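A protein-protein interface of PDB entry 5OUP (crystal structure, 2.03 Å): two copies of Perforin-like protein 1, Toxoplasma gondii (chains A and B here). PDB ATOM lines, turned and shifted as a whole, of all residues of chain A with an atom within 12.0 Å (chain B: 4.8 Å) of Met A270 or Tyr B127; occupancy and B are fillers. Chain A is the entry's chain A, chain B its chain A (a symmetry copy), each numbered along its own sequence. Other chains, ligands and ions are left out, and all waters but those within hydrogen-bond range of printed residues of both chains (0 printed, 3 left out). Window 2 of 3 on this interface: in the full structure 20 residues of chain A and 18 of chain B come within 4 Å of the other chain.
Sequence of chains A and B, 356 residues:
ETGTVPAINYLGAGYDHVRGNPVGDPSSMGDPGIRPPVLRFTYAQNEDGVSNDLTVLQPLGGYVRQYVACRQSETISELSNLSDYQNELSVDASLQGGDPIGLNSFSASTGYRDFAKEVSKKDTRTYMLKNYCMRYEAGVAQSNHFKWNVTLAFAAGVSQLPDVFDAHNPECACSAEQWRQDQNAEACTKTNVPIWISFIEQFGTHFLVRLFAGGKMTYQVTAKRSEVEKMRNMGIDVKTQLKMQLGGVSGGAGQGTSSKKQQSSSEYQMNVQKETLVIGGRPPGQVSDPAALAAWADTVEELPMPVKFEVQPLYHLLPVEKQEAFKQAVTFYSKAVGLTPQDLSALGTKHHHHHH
OG of Ser B77 lies within hydrogen-bond range of OD1 of Asn A271, 3.5 Å away.
The backbone carbonyl oxygen of Met A270 lies close to the backbone carbonyl oxygen of Ile B76, at 3.3 Å.
The backbone carbonyl oxygen (O) of Val A272 sits at hydrogen-bond distance from the backbone NH (N) of Ile B76, at 3.0 Å.
Positions printed for both chains: 125, 127 and 221.
Of the 7 pairs that touch across the chains among the printed residues, none has its exchanged pair printed and touching as well.
N of Lys A224 is in hydrogen-bond range of O of Asn A271.
OE2 of Glu B78 is in salt-bridge range of NH1 of Arg B125 (3.9 Å).
O of Val B221 lies within hydrogen-bond range of N of Tyr B127, at 2.7 Å.
The backbone NH (N) of Met B128 is in hydrogen-bond range of the backbone carbonyl oxygen (O) of Ser B77 (2.8 Å).
Of the 15 printed residues of chain A, 4 touch a printed residue of chain B.
Hydrophobic or aromatic side chains of chain A within 4 Å of the printed part of chain B: Met A270.
Of the printed residues of chain B, Met A270 touches Ile B76 (3.3 Å), Glu B78 (3.8 Å) and Tyr B127 (3.98 Å).
Of chain A, only Met A270 (3.98 Å) comes within 4 Å of Tyr B127.
Ile B76 touches three residues of chain A.
Of chain A, only Gln A269 (3.9 Å) and Met A270 (3.8 Å) come within 4 Å of Glu B78.
No residue of chain A comes within 4 Å of Leu B79.
No residue of chain A comes within 4 Å of Leu B129.
No residue of chain A comes within 4 Å of Gln B220.
No residue of chain A comes within 4 Å of Val B221.
Of the printed residues of chain B, Asn A271 touches Ile B76 (3.4 Å) and Ser B77 (3.5 Å).
Printed residues of chain B within 4 Å of Gln A269: Glu B78 (3.9 Å).
Of the printed residues of chain B, Val A272 touches Ile B76.
Thr A124 touches none of the printed residues of chain B.
The nearest residue of chain B that does not touch Met A270 is Ser B77 (4.4 Å).
The nearest residue of chain A that does not touch Tyr B127 is Gln A269 (7.6 Å).
Among the printed residues, merely in contact across the chains: Gln A269 with Glu B78 (3.9 Å), Met A270 with Glu B78 (3.8 Å), Met A270 with Tyr B127 (3.98 Å) and Asn A271 with Ile B76 (3.4 Å).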
ATOM      1  N   ASP A 123      -4.755  12.774  -9.996  1.00  0.00           N
ATOM      2  CA  ASP A 123      -4.222  11.686  -9.187  1.00  0.00           C
ATOM      3  C   ASP A 123      -3.184  10.848  -9.920  1.00  0.00           C
ATOM      4  O   ASP A 123      -2.709   9.854  -9.360  1.00  0.00           O
ATOM      5  CB  ASP A 123      -5.358  10.775  -8.719  1.00  0.00           C
ATOM      6  CG  ASP A 123      -6.159  10.214  -9.873  1.00  0.00           C
ATOM      7  OD1 ASP A 123      -6.388  10.960 -10.848  1.00  0.00           O
ATOM      8  OD2 ASP A 123      -6.554   9.032  -9.812  1.00  0.00           O
ATOM      9  N   THR A 124      -2.835  11.197 -11.156  1.00  0.00           N
ATOM     10  CA  THR A 124      -1.846  10.455 -11.924  1.00  0.00           C
ATOM     11  C   THR A 124      -0.846  11.418 -12.548  1.00  0.00           C
ATOM     12  O   THR A 124      -1.123  12.607 -12.735  1.00  0.00           O
ATOM     13  CB  THR A 124      -2.487   9.604 -13.036  1.00  0.00           C
ATOM     14  OG1 THR A 124      -3.045  10.463 -14.040  1.00  0.00           O
ATOM     15  CG2 THR A 124      -3.581   8.702 -12.473  1.00  0.00           C
ATOM     16  N   ARG A 125       0.328  10.878 -12.876  1.00  0.00           N
ATOM     17  CA  ARG A 125       1.388  11.634 -13.526  1.00  0.00           C
ATOM     18  C   ARG A 125       1.899  10.833 -14.713  1.00  0.00           C
ATOM     19  O   ARG A 125       2.115   9.622 -14.600  1.00  0.00           O
ATOM     20  CB  ARG A 125       2.527  11.942 -12.546  1.00  0.00           C
ATOM     21  CG  ARG A 125       3.340  13.183 -12.892  1.00  0.00           C
ATOM     22  CD  ARG A 125       2.443  14.375 -13.218  1.00  0.00           C
ATOM     23  NE  ARG A 125       1.324  14.511 -12.286  1.00  0.00           N
ATOM     24  CZ  ARG A 125       1.305  15.334 -11.243  1.00  0.00           C
ATOM     25  NH1 ARG A 125       2.348  16.112 -10.990  1.00  0.00           N
ATOM     26  NH2 ARG A 125       0.238  15.381 -10.456  1.00  0.00           N
ATOM     27  N   TYR A 127       4.616  10.444 -18.081  1.00  0.00           N
ATOM     28  CA  TYR A 127       5.917  10.741 -18.657  1.00  0.00           C
ATOM     29  C   TYR A 127       5.932  10.258 -20.100  1.00  0.00           C
ATOM     30  O   TYR A 127       5.244   9.294 -20.449  1.00  0.00           O
ATOM     31  CB  TYR A 127       7.049  10.061 -17.863  1.00  0.00           C
ATOM     32  CG  TYR A 127       6.991  10.325 -16.374  1.00  0.00           C
ATOM     33  CD1 TYR A 127       6.175   9.564 -15.543  1.00  0.00           C
ATOM     34  CD2 TYR A 127       7.750  11.337 -15.799  1.00  0.00           C
ATOM     35  CE1 TYR A 127       6.115   9.806 -14.182  1.00  0.00           C
ATOM     36  CE2 TYR A 127       7.697  11.584 -14.439  1.00  0.00           C
ATOM     37  CZ  TYR A 127       6.879  10.816 -13.636  1.00  0.00           C
ATOM     38  OH  TYR A 127       6.824  11.059 -12.283  1.00  0.00           O
ATOM     39  N   VAL A 221       4.075   6.745 -20.146  1.00  0.00           N
ATOM     40  CA  VAL A 221       4.021   5.997 -18.898  1.00  0.00           C
ATOM     41  C   VAL A 221       3.275   6.838 -17.877  1.00  0.00           C
ATOM     42  O   VAL A 221       3.668   7.975 -17.590  1.00  0.00           O
ATOM     43  CB  VAL A 221       5.425   5.633 -18.394  1.00  0.00           C
ATOM     44  CG1 VAL A 221       5.330   4.785 -17.131  1.00  0.00           C
ATOM     45  CG2 VAL A 221       6.198   4.898 -19.478  1.00  0.00           C
ATOM     46  N   THR A 222       2.203   6.278 -17.328  1.00  0.00           N
ATOM     47  CA  THR A 222       1.371   6.952 -16.344  1.00  0.00           C
ATOM     48  C   THR A 222       1.460   6.194 -15.030  1.00  0.00           C
ATOM     49  O   THR A 222       1.282   4.971 -15.001  1.00  0.00           O
ATOM     50  CB  THR A 222      -0.082   7.034 -16.820  1.00  0.00           C
ATOM     51  OG1 THR A 222      -0.133   7.709 -18.082  1.00  0.00           O
ATOM     52  CG2 THR A 222      -0.933   7.787 -15.816  1.00  0.00           C
ATOM     53  N   ALA A 223       1.750   6.916 -13.952  1.00  0.00           N
ATOM     54  CA  ALA A 223       1.854   6.338 -12.622  1.00  0.00           C
ATOM     55  C   ALA A 223       0.822   6.982 -11.710  1.00  0.00           C
ATOM     56  O   ALA A 223       0.626   8.201 -11.743  1.00  0.00           O
ATOM     57  CB  ALA A 223       3.261   6.522 -12.041  1.00  0.00           C
ATOM     58  N   LYS A 224       0.156   6.156 -10.908  1.00  0.00           N
ATOM     59  CA  LYS A 224      -0.840   6.659  -9.973  1.00  0.00           C
ATOM     60  C   LYS A 224      -0.161   7.480  -8.884  1.00  0.00           C
ATOM     61  O   LYS A 224       0.846   7.053  -8.311  1.00  0.00           O
ATOM     62  CB  LYS A 224      -1.616   5.499  -9.356  1.00  0.00           C
ATOM     63  CG  LYS A 224      -2.949   5.884  -8.742  1.00  0.00           C
ATOM     64  CD  LYS A 224      -4.060   5.861  -9.779  1.00  0.00           C
ATOM     65  CE  LYS A 224      -5.415   6.102  -9.137  1.00  0.00           C
ATOM     66  NZ  LYS A 224      -5.687   5.145  -8.028  1.00  0.00           N
ATOM     67  N   ARG A 225      -0.714   8.659  -8.607  1.00  0.00           N
ATOM     68  CA  ARG A 225      -0.184   9.570  -7.590  1.00  0.00           C
ATOM     69  C   ARG A 225       1.285   9.906  -7.834  1.00  0.00           C
ATOM     70  O   ARG A 225       1.679  11.072  -7.797  1.00  0.00           O
ATOM     71  CB  ARG A 225      -0.362   8.977  -6.189  1.00  0.00           C
ATOM     72  CG  ARG A 225       0.297   9.786  -5.087  1.00  0.00           C
ATOM     73  CD  ARG A 225       0.886   8.871  -4.028  1.00  0.00           C
ATOM     74  NE  ARG A 225       1.566   7.730  -4.633  1.00  0.00           N
ATOM     75  CZ  ARG A 225       2.790   7.773  -5.151  1.00  0.00           C
ATOM     76  NH1 ARG A 225       3.479   8.907  -5.140  1.00  0.00           N
ATOM     77  NH2 ARG A 225       3.325   6.683  -5.684  1.00  0.00           N
ATOM     78  N   GLN A 269       0.802   0.292  -3.532  1.00  0.00           N
ATOM     79  CA  GLN A 269       0.352   0.269  -4.919  1.00  0.00           C
ATOM     80  C   GLN A 269       1.414   0.818  -5.871  1.00  0.00           C
ATOM     81  O   GLN A 269       1.766   1.995  -5.807  1.00  0.00           O
ATOM     82  CB  GLN A 269      -0.943   1.072  -5.079  1.00  0.00           C
ATOM     83  CG  GLN A 269      -2.146   0.482  -4.367  1.00  0.00           C
ATOM     84  CD  GLN A 269      -3.434   1.204  -4.717  1.00  0.00           C
ATOM     85  OE1 GLN A 269      -3.553   2.416  -4.531  1.00  0.00           O
ATOM     86  NE2 GLN A 269      -4.403   0.462  -5.242  1.00  0.00           N
ATOM     87  N   MET A 270       1.915  -0.040  -6.758  1.00  0.00           N
ATOM     88  CA  MET A 270       2.876   0.348  -7.791  1.00  0.00           C
ATOM     89  C   MET A 270       2.188   0.586  -9.127  1.00  0.00           C
ATOM     90  O   MET A 270       2.721   0.247 -10.189  1.00  0.00           O
ATOM     91  CB  MET A 270       3.965  -0.712  -7.927  1.00  0.00           C
ATOM     92  CG  MET A 270       3.444  -2.107  -8.235  1.00  0.00           C
ATOM     93  SD  MET A 270       4.781  -3.287  -8.487  1.00  0.00           S
ATOM     94  CE  MET A 270       5.759  -2.420  -9.712  1.00  0.00           C
ATOM     95  N   ASN A 271       0.994   1.178  -9.087  1.00  0.00           N
ATOM     96  CA  ASN A 271       0.125   1.326 -10.249  1.00  0.00           C
ATOM     97  C   ASN A 271       0.801   2.114 -11.366  1.00  0.00           C
ATOM     98  O   ASN A 271       0.956   3.336 -11.268  1.00  0.00           O
ATOM     99  CB  ASN A 271      -1.182   2.005  -9.820  1.00  0.00           C
ATOM    100  CG  ASN A 271      -2.344   1.692 -10.744  1.00  0.00           C
ATOM    101  OD1 ASN A 271      -2.190   1.639 -11.962  1.00  0.00           O
ATOM    102  ND2 ASN A 271      -3.521   1.487 -10.162  1.00  0.00           N
ATOM    103  N   VAL A 272       1.205   1.423 -12.432  1.00  0.00           N
ATOM    104  CA  VAL A 272       1.869   2.039 -13.575  1.00  0.00           C
ATOM    105  C   VAL A 272       1.225   1.517 -14.853  1.00  0.00           C
ATOM    106  O   VAL A 272       0.994   0.310 -14.990  1.00  0.00           O
ATOM    107  CB  VAL A 272       3.385   1.756 -13.575  1.00  0.00           C
ATOM    108  CG1 VAL A 272       4.022   2.248 -14.864  1.00  0.00           C
ATOM    109  CG2 VAL A 272       4.051   2.412 -12.375  1.00  0.00           C
ATOM    110  N   GLN A 273       0.934   2.426 -15.782  1.00  0.00           N
ATOM    111  CA  GLN A 273       0.415   2.097 -17.104  1.00  0.00           C
ATOM    112  C   GLN A 273       1.393   2.587 -18.163  1.00  0.00           C
ATOM    113  O   GLN A 273       1.976   3.666 -18.026  1.00  0.00           O
ATOM    114  CB  GLN A 273      -0.961   2.735 -17.347  1.00  0.00           C
ATOM    115  CG  GLN A 273      -2.080   2.223 -16.454  1.00  0.00           C
ATOM    116  CD  GLN A 273      -2.090   2.863 -15.079  1.00  0.00           C
ATOM    117  OE1 GLN A 273      -1.641   3.995 -14.902  1.00  0.00           O
ATOM    118  NE2 GLN A 273      -2.607   2.136 -14.096  1.00  0.00           N
ATOM    119  N   LYS A 274       1.564   1.799 -19.223  1.00  0.00           N
ATOM    120  CA  LYS A 274       2.461   2.167 -20.311  1.00  0.00           C
ATOM    121  C   LYS A 274       1.796   1.875 -21.646  1.00  0.00           C
ATOM    122  O   LYS A 274       1.337   0.754 -21.879  1.00  0.00           O
ATOM    123  CB  LYS A 274       3.793   1.417 -20.219  1.00  0.00           C
ATOM    124  CG  LYS A 274       4.766   1.764 -21.339  1.00  0.00           C
ATOM    125  CD  LYS A 274       6.131   1.136 -21.108  1.00  0.00           C
ATOM    126  CE  LYS A 274       6.091  -0.371 -21.296  1.00  0.00           C
ATOM    127  NZ  LYS A 274       5.807  -0.734 -22.709  1.00  0.00           N
ATOM    128  N   ILE B  76       0.704  -2.611 -14.620  1.00  0.00           N
ATOM    129  CA  ILE B  76       1.054  -3.436 -13.468  1.00  0.00           C
ATOM    130  C   ILE B  76       0.532  -2.755 -12.213  1.00  0.00           C
ATOM    131  O   ILE B  76       0.645  -1.534 -12.060  1.00  0.00           O
ATOM    132  CB  ILE B  76       2.573  -3.690 -13.366  1.00  0.00           C
ATOM    133  CG1 ILE B  76       2.878  -4.575 -12.155  1.00  0.00           C
ATOM    134  CG2 ILE B  76       3.344  -2.381 -13.279  1.00  0.00           C
ATOM    135  CD1 ILE B  76       4.339  -4.915 -11.997  1.00  0.00           C
ATOM    136  N   SER B  77      -0.048  -3.547 -11.316  1.00  0.00           N
ATOM    137  CA  SER B  77      -0.633  -3.014 -10.096  1.00  0.00           C
ATOM    138  C   SER B  77      -0.437  -4.013  -8.969  1.00  0.00           C
ATOM    139  O   SER B  77      -0.597  -5.218  -9.170  1.00  0.00           O
ATOM    140  CB  SER B  77      -2.128  -2.718 -10.273  1.00  0.00           C
ATOM    141  OG  SER B  77      -2.344  -1.768 -11.299  1.00  0.00           O
ATOM    142  N   GLU B  78      -0.095  -3.506  -7.789  1.00  0.00           N
ATOM    143  CA  GLU B  78      -0.129  -4.314  -6.578  1.00  0.00           C
ATOM    144  C   GLU B  78      -1.540  -4.253  -6.008  1.00  0.00           C
ATOM    145  O   GLU B  78      -2.058  -3.163  -5.740  1.00  0.00           O
ATOM    146  CB  GLU B  78       0.891  -3.832  -5.549  1.00  0.00           C
ATOM    147  CG  GLU B  78       0.816  -4.593  -4.232  1.00  0.00           C
ATOM    148  CD  GLU B  78       1.957  -4.264  -3.292  1.00  0.00           C
ATOM    149  OE1 GLU B  78       2.906  -3.576  -3.724  1.00  0.00           O
ATOM    150  OE2 GLU B  78       1.904  -4.691  -2.121  1.00  0.00           O
ATOM    151  N   LEU B  79      -2.159  -5.415  -5.840  1.00  0.00           N
ATOM    152  CA  LEU B  79      -3.526  -5.514  -5.333  1.00  0.00           C
ATOM    153  C   LEU B  79      -3.461  -5.851  -3.847  1.00  0.00           C
ATOM    154  O   LEU B  79      -3.369  -7.020  -3.468  1.00  0.00           O
ATOM    155  CB  LEU B  79      -4.309  -6.561  -6.116  1.00  0.00           C
ATOM    156  CG  LEU B  79      -4.322  -6.352  -7.630  1.00  0.00           C
ATOM    157  CD1 LEU B  79      -5.066  -7.485  -8.318  1.00  0.00           C
ATOM    158  CD2 LEU B  79      -4.952  -5.011  -7.959  1.00  0.00           C
ATOM    159  N   ARG B 125       1.327 -11.588  -1.151  1.00  0.00           N
ATOM    160  CA  ARG B 125       1.073 -10.345  -1.867  1.00  0.00           C
ATOM    161  C   ARG B 125       0.877 -10.665  -3.340  1.00  0.00           C
ATOM    162  O   ARG B 125       1.637 -11.451  -3.915  1.00  0.00           O
ATOM    163  CB  ARG B 125       2.227  -9.352  -1.674  1.00  0.00           C
ATOM    164  CG  ARG B 125       1.831  -7.890  -1.824  1.00  0.00           C
ATOM    165  CD  ARG B 125       0.569  -7.559  -1.030  1.00  0.00           C
ATOM    166  NE  ARG B 125       0.576  -8.147   0.310  1.00  0.00           N
ATOM    167  CZ  ARG B 125       0.920  -7.499   1.417  1.00  0.00           C
ATOM    168  NH1 ARG B 125       1.287  -6.227   1.358  1.00  0.00           N
ATOM    169  NH2 ARG B 125       0.892  -8.127   2.586  1.00  0.00           N
ATOM    170  N   THR B 126      -0.145 -10.067  -3.944  1.00  0.00           N
ATOM    171  CA  THR B 126      -0.519 -10.366  -5.318  1.00  0.00           C
ATOM    172  C   THR B 126      -0.393  -9.118  -6.181  1.00  0.00           C
ATOM    173  O   THR B 126      -0.735  -8.011  -5.752  1.00  0.00           O
ATOM    174  CB  THR B 126      -1.948 -10.917  -5.404  1.00  0.00           C
ATOM    175  OG1 THR B 126      -2.884  -9.842  -5.268  1.00  0.00           O
ATOM    176  CG2 THR B 126      -2.197 -11.927  -4.296  1.00  0.00           C
ATOM    177  N   TYR B 127       0.107  -9.312  -7.397  1.00  0.00           N
ATOM    178  CA  TYR B 127       0.248  -8.266  -8.395  1.00  0.00           C
ATOM    179  C   TYR B 127      -0.542  -8.666  -9.633  1.00  0.00           C
ATOM    180  O   TYR B 127      -0.703  -9.855  -9.921  1.00  0.00           O
ATOM    181  CB  TYR B 127       1.726  -8.040  -8.765  1.00  0.00           C
ATOM    182  CG  TYR B 127       2.628  -7.835  -7.567  1.00  0.00           C
ATOM    183  CD1 TYR B 127       3.141  -8.917  -6.863  1.00  0.00           C
ATOM    184  CD2 TYR B 127       2.964  -6.556  -7.139  1.00  0.00           C
ATOM    185  CE1 TYR B 127       3.961  -8.734  -5.763  1.00  0.00           C
ATOM    186  CE2 TYR B 127       3.785  -6.363  -6.041  1.00  0.00           C
ATOM    187  CZ  TYR B 127       4.280  -7.455  -5.359  1.00  0.00           C
ATOM    188  OH  TYR B 127       5.096  -7.267  -4.267  1.00  0.00           O
ATOM    189  N   MET B 128      -1.043  -7.675 -10.364  1.00  0.00           N
ATOM    190  CA  MET B 128      -1.741  -7.930 -11.617  1.00  0.00           C
ATOM    191  C   MET B 128      -1.012  -7.233 -12.757  1.00  0.00           C
ATOM    192  O   MET B 128      -0.761  -6.025 -12.691  1.00  0.00           O
ATOM    193  CB  MET B 128      -3.197  -7.465 -11.554  1.00  0.00           C
ATOM    194  CG  MET B 128      -4.095  -8.161 -12.566  1.00  0.00           C
ATOM    195  SD  MET B 128      -5.680  -7.325 -12.712  1.00  0.00           S
ATOM    196  CE  MET B 128      -5.076  -5.680 -13.023  1.00  0.00           C
ATOM    197  N   LEU B 129      -0.675  -7.999 -13.793  1.00  0.00           N
ATOM    198  CA  LEU B 129       0.012  -7.493 -14.978  1.00  0.00           C
ATOM    199  C   LEU B 129      -0.902  -7.688 -16.180  1.00  0.00           C
ATOM    200  O   LEU B 129      -1.155  -8.824 -16.591  1.00  0.00           O
ATOM    201  CB  LEU B 129       1.342  -8.219 -15.191  1.00  0.00           C
ATOM    202  CG  LEU B 129       2.524  -7.905 -14.278  1.00  0.00           C
ATOM    203  CD1 LEU B 129       3.325  -9.165 -14.000  1.00  0.00           C
ATOM    204  CD2 LEU B 129       3.408  -6.862 -14.938  1.00  0.00           C
ATOM    205  N   TYR B 219      -1.668 -11.504 -16.113  1.00  0.00           N
ATOM    206  CA  TYR B 219      -1.004 -12.379 -15.158  1.00  0.00           C
ATOM    207  C   TYR B 219      -1.297 -11.888 -13.750  1.00  0.00           C
ATOM    208  O   TYR B 219      -1.085 -10.711 -13.441  1.00  0.00           O
ATOM    209  CB  TYR B 219       0.507 -12.418 -15.395  1.00  0.00           C
ATOM    210  CG  TYR B 219       0.899 -12.727 -16.816  1.00  0.00           C
ATOM    211  CD1 TYR B 219       0.802 -14.016 -17.319  1.00  0.00           C
ATOM    212  CD2 TYR B 219       1.373 -11.730 -17.657  1.00  0.00           C
ATOM    213  CE1 TYR B 219       1.159 -14.303 -18.626  1.00  0.00           C
ATOM    214  CE2 TYR B 219       1.732 -12.005 -18.962  1.00  0.00           C
ATOM    215  CZ  TYR B 219       1.623 -13.293 -19.442  1.00  0.00           C
ATOM    216  OH  TYR B 219       1.981 -13.571 -20.741  1.00  0.00           O
ATOM    217  N   GLN B 220      -1.794 -12.782 -12.906  1.00  0.00           N
ATOM    218  CA  GLN B 220      -1.954 -12.509 -11.484  1.00  0.00           C
ATOM    219  C   GLN B 220      -0.866 -13.283 -10.753  1.00  0.00           C
ATOM    220  O   GLN B 220      -0.873 -14.520 -10.737  1.00  0.00           O
ATOM    221  CB  GLN B 220      -3.357 -12.875 -11.009  1.00  0.00           C
ATOM    222  CG  GLN B 220      -4.382 -11.871 -11.513  1.00  0.00           C
ATOM    223  CD  GLN B 220      -5.812 -12.256 -11.210  1.00  0.00           C
ATOM    224  OE1 GLN B 220      -6.076 -13.185 -10.447  1.00  0.00           O
ATOM    225  NE2 GLN B 220      -6.748 -11.535 -11.815  1.00  0.00           N
ATOM    226  N   VAL B 221       0.084 -12.552 -10.180  1.00  0.00           N
ATOM    227  CA  VAL B 221       1.291 -13.126  -9.599  1.00  0.00           C
ATOM    228  C   VAL B 221       1.228 -12.932  -8.094  1.00  0.00           C
ATOM    229  O   VAL B 221       1.107 -11.800  -7.610  1.00  0.00           O
ATOM    230  CB  VAL B 221       2.560 -12.491 -10.186  1.00  0.00           C
ATOM    231  CG1 VAL B 221       3.801 -13.167  -9.616  1.00  0.00           C
ATOM    232  CG2 VAL B 221       2.543 -12.588 -11.703  1.00  0.00           C
